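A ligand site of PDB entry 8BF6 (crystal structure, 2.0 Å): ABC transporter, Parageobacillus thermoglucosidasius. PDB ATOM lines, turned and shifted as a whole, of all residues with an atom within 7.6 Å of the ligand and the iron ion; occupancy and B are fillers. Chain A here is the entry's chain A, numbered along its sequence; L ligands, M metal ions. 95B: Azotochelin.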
ATOM      1  N   ASN A  65      16.634 -20.035 -10.201  1.00  0.00           N
ATOM      2  CA  ASN A  65      17.542 -20.954  -9.517  1.00  0.00           C
ATOM      3  C   ASN A  65      18.738 -20.224  -8.884  1.00  0.00           C
ATOM      4  O   ASN A  65      19.744 -20.858  -8.654  1.00  0.00           O
ATOM      5  CB  ASN A  65      18.115 -22.007 -10.471  1.00  0.00           C
ATOM      6  CG  ASN A  65      17.076 -22.940 -11.037  1.00  0.00           C
ATOM      7  OD1 ASN A  65      16.793 -22.914 -12.238  1.00  0.00           O
ATOM      8  ND2 ASN A  65      16.465 -23.715 -10.169  1.00  0.00           N
ATOM      9  N   GLY A  83      14.874 -20.476 -15.968  1.00  0.00           N
ATOM     10  CA  GLY A  83      15.567 -21.412 -15.092  1.00  0.00           C
ATOM     11  C   GLY A  83      16.781 -21.992 -15.807  1.00  0.00           C
ATOM     12  O   GLY A  83      16.826 -21.965 -17.030  1.00  0.00           O
ATOM     13  N   LEU A  84      17.753 -22.473 -15.015  1.00  0.00           N
ATOM     14  CA  LEU A  84      18.891 -23.239 -15.506  1.00  0.00           C
ATOM     15  C   LEU A  84      18.463 -24.304 -16.523  1.00  0.00           C
ATOM     16  O   LEU A  84      19.134 -24.508 -17.536  1.00  0.00           O
ATOM     17  CB  LEU A  84      19.561 -23.936 -14.325  1.00  0.00           C
ATOM     18  CG  LEU A  84      20.377 -23.047 -13.394  1.00  0.00           C
ATOM     19  CD1 LEU A  84      20.790 -23.827 -12.157  1.00  0.00           C
ATOM     20  CD2 LEU A  84      21.606 -22.508 -14.102  1.00  0.00           C
ATOM     21  N   MET A  85      17.355 -24.985 -16.233  1.00  0.00           N
ATOM     22  CA  MET A  85      16.906 -26.072 -17.087  1.00  0.00           C
ATOM     23  C   MET A  85      15.739 -25.626 -17.975  1.00  0.00           C
ATOM     24  O   MET A  85      15.193 -26.451 -18.676  1.00  0.00           O
ATOM     25  CB  MET A  85      16.434 -27.267 -16.254  1.00  0.00           C
ATOM     26  CG  MET A  85      17.495 -27.780 -15.292  1.00  0.00           C
ATOM     27  SD  MET A  85      18.949 -28.459 -16.124  1.00  0.00           S
ATOM     28  CE  MET A  85      19.465 -29.575 -14.831  1.00  0.00           C
ATOM     29  N   GLU A  86      15.328 -24.350 -17.917  1.00  0.00           N
ATOM     30  CA  GLU A  86      14.123 -23.896 -18.587  1.00  0.00           C
ATOM     31  C   GLU A  86      14.358 -22.446 -19.025  1.00  0.00           C
ATOM     32  O   GLU A  86      13.864 -21.522 -18.376  1.00  0.00           O
ATOM     33  CB  GLU A  86      12.900 -23.952 -17.662  1.00  0.00           C
ATOM     34  CG  GLU A  86      12.539 -25.353 -17.183  1.00  0.00           C
ATOM     35  CD  GLU A  86      11.392 -25.370 -16.189  1.00  0.00           C
ATOM     36  OE1 GLU A  86      10.874 -26.477 -15.916  1.00  0.00           O
ATOM     37  OE2 GLU A  86      11.026 -24.295 -15.688  1.00  0.00           O
ATOM     38  N   SER A 103      26.754 -23.459 -19.677  1.00  0.00           N
ATOM     39  CA  SER A 103      27.616 -24.560 -19.284  1.00  0.00           C
ATOM     40  C   SER A 103      26.824 -25.861 -19.382  1.00  0.00           C
ATOM     41  O   SER A 103      25.879 -25.937 -20.171  1.00  0.00           O
ATOM     42  CB  SER A 103      28.196 -24.310 -17.899  1.00  0.00           C
ATOM     43  OG  SER A 103      27.143 -24.230 -16.942  1.00  0.00           O
ATOM     44  N   GLY A 104      27.205 -26.864 -18.580  1.00  0.00           N
ATOM     45  CA  GLY A 104      26.779 -28.250 -18.731  1.00  0.00           C
ATOM     46  C   GLY A 104      25.263 -28.453 -18.789  1.00  0.00           C
ATOM     47  O   GLY A 104      24.790 -29.195 -19.634  1.00  0.00           O
ATOM     48  N   ARG A 105      24.509 -27.806 -17.894  1.00  0.00           N
ATOM     49  CA  ARG A 105      23.061 -27.984 -17.837  1.00  0.00           C
ATOM     50  C   ARG A 105      22.364 -27.567 -19.145  1.00  0.00           C
ATOM     51  O   ARG A 105      21.248 -28.009 -19.397  1.00  0.00           O
ATOM     52  CB  ARG A 105      22.499 -27.173 -16.659  1.00  0.00           C
ATOM     53  CG  ARG A 105      22.850 -27.720 -15.276  1.00  0.00           C
ATOM     54  CD  ARG A 105      22.132 -27.003 -14.145  1.00  0.00           C
ATOM     55  NE  ARG A 105      22.356 -27.664 -12.868  1.00  0.00           N
ATOM     56  CZ  ARG A 105      23.302 -27.308 -11.995  1.00  0.00           C
ATOM     57  NH1 ARG A 105      23.365 -27.844 -10.783  1.00  0.00           N
ATOM     58  NH2 ARG A 105      24.172 -26.378 -12.333  1.00  0.00           N
ATOM     59  N   GLN A 106      22.979 -26.673 -19.948  1.00  0.00           N
ATOM     60  CA  GLN A 106      22.368 -26.183 -21.180  1.00  0.00           C
ATOM     61  C   GLN A 106      23.041 -26.726 -22.442  1.00  0.00           C
ATOM     62  O   GLN A 106      22.689 -26.312 -23.545  1.00  0.00           O
ATOM     63  CB  GLN A 106      22.457 -24.657 -21.258  1.00  0.00           C
ATOM     64  CG  GLN A 106      21.750 -23.913 -20.143  1.00  0.00           C
ATOM     65  CD  GLN A 106      22.595 -23.774 -18.891  1.00  0.00           C
ATOM     66  OE1 GLN A 106      23.823 -23.641 -18.960  1.00  0.00           O
ATOM     67  NE2 GLN A 106      21.940 -23.774 -17.749  1.00  0.00           N
ATOM     68  N   ALA A 107      24.001 -27.672 -22.313  1.00  0.00           N
ATOM     69  CA  ALA A 107      24.801 -28.066 -23.459  1.00  0.00           C
ATOM     70  C   ALA A 107      23.903 -28.552 -24.603  1.00  0.00           C
ATOM     71  O   ALA A 107      24.151 -28.203 -25.747  1.00  0.00           O
ATOM     72  CB  ALA A 107      25.822 -29.101 -23.053  1.00  0.00           C
ATOM     73  N   ASN A 108      22.833 -29.294 -24.265  1.00  0.00           N
ATOM     74  CA  ASN A 108      21.842 -29.766 -25.225  1.00  0.00           C
ATOM     75  C   ASN A 108      21.216 -28.658 -26.045  1.00  0.00           C
ATOM     76  O   ASN A 108      20.750 -28.907 -27.145  1.00  0.00           O
ATOM     77  CB  ASN A 108      20.672 -30.478 -24.527  1.00  0.00           C
ATOM     78  CG  ASN A 108      20.902 -31.966 -24.426  1.00  0.00           C
ATOM     79  OD1 ASN A 108      21.886 -32.473 -24.949  1.00  0.00           O
ATOM     80  ND2 ASN A 108      19.980 -32.671 -23.797  1.00  0.00           N
ATOM     81  N   LEU A 179      25.829 -37.195  -2.080  1.00  0.00           N
ATOM     82  CA  LEU A 179      24.764 -36.255  -2.406  1.00  0.00           C
ATOM     83  C   LEU A 179      23.410 -36.829  -1.989  1.00  0.00           C
ATOM     84  O   LEU A 179      23.132 -37.996  -2.272  1.00  0.00           O
ATOM     85  CB  LEU A 179      24.833 -36.012  -3.921  1.00  0.00           C
ATOM     86  CG  LEU A 179      23.762 -35.090  -4.518  1.00  0.00           C
ATOM     87  CD1 LEU A 179      24.391 -34.015  -5.388  1.00  0.00           C
ATOM     88  CD2 LEU A 179      22.740 -35.917  -5.304  1.00  0.00           C
ATOM     89  N   THR A 181      19.201 -36.653  -2.237  1.00  0.00           N
ATOM     90  CA  THR A 181      17.998 -36.213  -2.925  1.00  0.00           C
ATOM     91  C   THR A 181      16.893 -37.246  -2.728  1.00  0.00           C
ATOM     92  O   THR A 181      17.138 -38.429  -2.937  1.00  0.00           O
ATOM     93  CB  THR A 181      18.154 -36.104  -4.455  1.00  0.00           C
ATOM     94  OG1 THR A 181      19.493 -35.776  -4.804  1.00  0.00           O
ATOM     95  CG2 THR A 181      17.195 -35.098  -5.059  1.00  0.00           C
ATOM     96  N   TYR A 188      30.352 -39.678  -5.189  1.00  0.00           N
ATOM     97  CA  TYR A 188      31.332 -39.114  -6.087  1.00  0.00           C
ATOM     98  C   TYR A 188      32.727 -39.323  -5.537  1.00  0.00           C
ATOM     99  O   TYR A 188      32.936 -39.123  -4.339  1.00  0.00           O
ATOM    100  CB  TYR A 188      31.179 -37.598  -6.226  1.00  0.00           C
ATOM    101  CG  TYR A 188      29.855 -37.130  -6.757  1.00  0.00           C
ATOM    102  CD1 TYR A 188      28.715 -37.191  -5.988  1.00  0.00           C
ATOM    103  CD2 TYR A 188      29.753 -36.640  -8.050  1.00  0.00           C
ATOM    104  CE1 TYR A 188      27.492 -36.755  -6.459  1.00  0.00           C
ATOM    105  CE2 TYR A 188      28.543 -36.191  -8.554  1.00  0.00           C
ATOM    106  CZ  TYR A 188      27.412 -36.263  -7.753  1.00  0.00           C
ATOM    107  OH  TYR A 188      26.223 -35.798  -8.209  1.00  0.00           O
ATOM    108  N   ARG A 193      32.436 -34.592 -10.398  1.00  0.00           N
ATOM    109  CA  ARG A 193      31.923 -33.246 -10.275  1.00  0.00           C
ATOM    110  C   ARG A 193      32.442 -32.580  -8.995  1.00  0.00           C
ATOM    111  O   ARG A 193      32.608 -31.365  -8.955  1.00  0.00           O
ATOM    112  CB  ARG A 193      30.407 -33.414 -10.291  1.00  0.00           C
ATOM    113  CG  ARG A 193      29.618 -32.151 -10.014  1.00  0.00           C
ATOM    114  CD  ARG A 193      28.167 -32.547  -9.906  1.00  0.00           C
ATOM    115  NE  ARG A 193      27.399 -31.334  -9.957  1.00  0.00           N
ATOM    116  CZ  ARG A 193      26.149 -31.233 -10.404  1.00  0.00           C
ATOM    117  NH1 ARG A 193      25.452 -32.306 -10.758  1.00  0.00           N
ATOM    118  NH2 ARG A 193      25.608 -30.039 -10.506  1.00  0.00           N
ATOM    119  N   THR A 214      26.727 -37.466 -13.358  1.00  0.00           N
ATOM    120  CA  THR A 214      26.305 -36.103 -13.053  1.00  0.00           C
ATOM    121  C   THR A 214      25.706 -36.016 -11.657  1.00  0.00           C
ATOM    122  O   THR A 214      26.040 -35.102 -10.903  1.00  0.00           O
ATOM    123  CB  THR A 214      25.266 -35.629 -14.079  1.00  0.00           C
ATOM    124  OG1 THR A 214      26.005 -35.521 -15.291  1.00  0.00           O
ATOM    125  CG2 THR A 214      24.635 -34.286 -13.743  1.00  0.00           C
ATOM    126  N   HIS A 215      24.754 -36.926 -11.379  1.00  0.00           N
ATOM    127  CA  HIS A 215      24.011 -36.910 -10.129  1.00  0.00           C
ATOM    128  C   HIS A 215      24.496 -38.014  -9.194  1.00  0.00           C
ATOM    129  O   HIS A 215      23.864 -38.260  -8.177  1.00  0.00           O
ATOM    130  CB  HIS A 215      22.513 -36.978 -10.419  1.00  0.00           C
ATOM    131  CG  HIS A 215      22.017 -35.702 -11.038  1.00  0.00           C
ATOM    132  ND1 HIS A 215      21.553 -35.663 -12.326  1.00  0.00           N
ATOM    133  CD2 HIS A 215      21.937 -34.442 -10.570  1.00  0.00           C
ATOM    134  CE1 HIS A 215      21.179 -34.419 -12.622  1.00  0.00           C
ATOM    135  NE2 HIS A 215      21.396 -33.657 -11.567  1.00  0.00           N
ATOM    136  N   ARG A 237      21.063 -31.734  -2.103  1.00  0.00           N
ATOM    137  CA  ARG A 237      20.546 -31.321  -3.390  1.00  0.00           C
ATOM    138  C   ARG A 237      19.145 -30.724  -3.226  1.00  0.00           C
ATOM    139  O   ARG A 237      18.862 -29.685  -3.810  1.00  0.00           O
ATOM    140  CB  ARG A 237      20.537 -32.485  -4.389  1.00  0.00           C
ATOM    141  CG  ARG A 237      20.014 -32.096  -5.768  1.00  0.00           C
ATOM    142  CD  ARG A 237      20.119 -33.227  -6.772  1.00  0.00           C
ATOM    143  NE  ARG A 237      19.557 -32.861  -8.064  1.00  0.00           N
ATOM    144  CZ  ARG A 237      18.324 -33.164  -8.449  1.00  0.00           C
ATOM    145  NH1 ARG A 237      17.511 -33.813  -7.640  1.00  0.00           N
ATOM    146  NH2 ARG A 237      17.900 -32.789  -9.637  1.00  0.00           N
ATOM    147  N   VAL A 240      18.448 -27.056  -2.713  1.00  0.00           N
ATOM    148  CA  VAL A 240      18.609 -26.060  -3.777  1.00  0.00           C
ATOM    149  C   VAL A 240      17.700 -26.361  -4.964  1.00  0.00           C
ATOM    150  O   VAL A 240      17.389 -25.426  -5.716  1.00  0.00           O
ATOM    151  CB  VAL A 240      20.066 -25.862  -4.233  1.00  0.00           C
ATOM    152  CG1 VAL A 240      20.882 -25.137  -3.185  1.00  0.00           C
ATOM    153  CG2 VAL A 240      20.733 -27.150  -4.681  1.00  0.00           C
ATOM    154  N   VAL A 241      17.309 -27.615  -5.180  1.00  0.00           N
ATOM    155  CA  VAL A 241      16.441 -27.964  -6.289  1.00  0.00           C
ATOM    156  C   VAL A 241      14.976 -27.798  -5.850  1.00  0.00           C
ATOM    157  O   VAL A 241      14.214 -27.150  -6.546  1.00  0.00           O
ATOM    158  CB  VAL A 241      16.773 -29.356  -6.852  1.00  0.00           C
ATOM    159  CG1 VAL A 241      15.653 -29.935  -7.719  1.00  0.00           C
ATOM    160  CG2 VAL A 241      18.100 -29.315  -7.604  1.00  0.00           C
ATOM    161  N   ALA A 242      14.619 -28.313  -4.672  1.00  0.00           N
ATOM    162  CA  ALA A 242      13.228 -28.328  -4.256  1.00  0.00           C
ATOM    163  C   ALA A 242      12.951 -27.226  -3.233  1.00  0.00           C
ATOM    164  O   ALA A 242      11.793 -27.015  -2.872  1.00  0.00           O
ATOM    165  CB  ALA A 242      12.899 -29.696  -3.709  1.00  0.00           C
ATOM    166  N   TYR A 276      26.602 -27.129  -5.696  1.00  0.00           N
ATOM    167  CA  TYR A 276      25.690 -27.795  -6.600  1.00  0.00           C
ATOM    168  C   TYR A 276      25.205 -26.809  -7.676  1.00  0.00           C
ATOM    169  O   TYR A 276      25.362 -27.120  -8.848  1.00  0.00           O
ATOM    170  CB  TYR A 276      24.534 -28.467  -5.856  1.00  0.00           C
ATOM    171  CG  TYR A 276      23.703 -29.309  -6.792  1.00  0.00           C
ATOM    172  CD1 TYR A 276      24.119 -30.567  -7.173  1.00  0.00           C
ATOM    173  CD2 TYR A 276      22.575 -28.779  -7.413  1.00  0.00           C
ATOM    174  CE1 TYR A 276      23.392 -31.331  -8.076  1.00  0.00           C
ATOM    175  CE2 TYR A 276      21.860 -29.516  -8.332  1.00  0.00           C
ATOM    176  CZ  TYR A 276      22.255 -30.800  -8.664  1.00  0.00           C
ATOM    177  OH  TYR A 276      21.516 -31.525  -9.566  1.00  0.00           O
ATOM    178  N   LEU A 277      24.630 -25.662  -7.283  1.00  0.00           N
ATOM    179  CA  LEU A 277      24.087 -24.698  -8.237  1.00  0.00           C
ATOM    180  C   LEU A 277      25.187 -23.954  -8.998  1.00  0.00           C
ATOM    181  O   LEU A 277      24.969 -23.533 -10.124  1.00  0.00           O
ATOM    182  CB  LEU A 277      23.201 -23.683  -7.526  1.00  0.00           C
ATOM    183  CG  LEU A 277      21.866 -24.192  -7.004  1.00  0.00           C
ATOM    184  CD1 LEU A 277      21.083 -23.044  -6.381  1.00  0.00           C
ATOM    185  CD2 LEU A 277      21.059 -24.903  -8.099  1.00  0.00           C
HETATM  186  OAH 95B L   1      19.315 -31.298 -11.761  1.00  0.00           O
HETATM  187  CBA 95B L   1      18.729 -30.077 -11.529  1.00  0.00           C
HETATM  188  CAY 95B L   1      19.667 -29.066 -11.310  1.00  0.00           C
HETATM  189  OAF 95B L   1      20.973 -29.494 -11.386  1.00  0.00           O
HETATM  190  CAL 95B L   1      19.252 -27.760 -11.074  1.00  0.00           C
HETATM  191  CAJ 95B L   1      17.880 -27.467 -11.074  1.00  0.00           C
HETATM  192  CAN 95B L   1      16.962 -28.459 -11.336  1.00  0.00           C
HETATM  193  CBC 95B L   1      17.357 -29.783 -11.559  1.00  0.00           C
HETATM  194  CAW 95B L   1      16.356 -30.835 -11.866  1.00  0.00           C
HETATM  195  OAC 95B L   1      15.166 -30.610 -11.717  1.00  0.00           O
HETATM  196  N   95B L   1      16.817 -31.958 -12.435  1.00  0.00           N
HETATM  197  CA  95B L   1      15.968 -32.936 -13.110  1.00  0.00           C
HETATM  198  C   95B L   1      15.227 -33.846 -12.107  1.00  0.00           C
HETATM  199  OXT 95B L   1      14.427 -34.669 -12.555  1.00  0.00           O
HETATM  200  O   95B L   1      15.498 -33.717 -10.907  1.00  0.00           O
HETATM  201  CB  95B L   1      16.809 -33.802 -14.059  1.00  0.00           C
HETATM  202  CAP 95B L   1      17.691 -32.998 -15.002  1.00  0.00           C
HETATM  203  CAO 95B L   1      18.580 -33.855 -15.884  1.00  0.00           C
HETATM  204  CAQ 95B L   1      19.516 -33.050 -16.770  1.00  0.00           C
HETATM  205  NAS 95B L   1      20.486 -32.283 -16.003  1.00  0.00           N
HETATM  206  CAV 95B L   1      21.685 -31.941 -16.475  1.00  0.00           C
HETATM  207  OAB 95B L   1      22.005 -32.172 -17.633  1.00  0.00           O
HETATM  208  CBB 95B L   1      22.735 -31.466 -15.534  1.00  0.00           C
HETATM  209  CAM 95B L   1      24.010 -31.162 -16.014  1.00  0.00           C
HETATM  210  CAI 95B L   1      24.994 -30.742 -15.162  1.00  0.00           C
HETATM  211  CAK 95B L   1      24.757 -30.632 -13.798  1.00  0.00           C
HETATM  212  CAX 95B L   1      23.509 -30.971 -13.287  1.00  0.00           C
HETATM  213  OAE 95B L   1      23.186 -30.891 -11.964  1.00  0.00           O
HETATM  214  CAZ 95B L   1      22.491 -31.369 -14.154  1.00  0.00           C
HETATM  215  OAG 95B L   1      21.281 -31.654 -13.567  1.00  0.00           O
HETATM  216 FE    FE M   1      21.323 -31.410 -11.577  1.00  0.00          FE
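The backbone carbonyl oxygen of Tyr 276 sits at hydrogen-bond distance from the guanidinium group of Arg 105 (2.9 Å). NE of Arg 237 sits close to OH of Tyr 276, at 2.8 Å. O of Tyr 276 lies within hydrogen-bond range of NH2 of Arg 193, 3.4 Å away. OH of Tyr 188 sits close to O of His 215, at 3.4 Å. O of Thr 214 is in hydrogen-bond range of NH1 of Arg 193 (2.9 Å). OH of Tyr 188 is in hydrogen-bond range of O of Thr 214.
The guanidinium group (NE) of Arg 105 sits close to an oxygen (OAF) of the ligand (2.7 Å). O of the ligand lies within salt-bridge range of NH2 of Arg 237 (2.9 Å). NH1 of Arg 193 sits close to OAE of the ligand, 2.9 Å away.
OAF of the ligand is bound to the iron ion (2.0 Å). OAE of the ligand binds the iron ion (2.0 Å). An oxygen (OAG) of the ligand binds the iron ion (2.0 Å). The iron ion is bound by an oxygen (OAH) of the ligand (2.0 Å). The side-chain hydroxyl (OH) of Tyr 276 binds the iron ion (2.0 Å). NE2 of His 215 is bound to the iron ion (2.2 Å). The iron ion has six donor atoms within binding distance.
CE of Met 85 touches OAG of the ligand, 3.0 Å away. Thr 214 touches the ligand. CG2 of Val 241 touches CAJ of the ligand, 3.9 Å away. Of the 23 residues printed, 8 come within 4 Å of the ligand. The nearest printed residue that does not touch the ligand is Gly 104 (4.1 Å).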
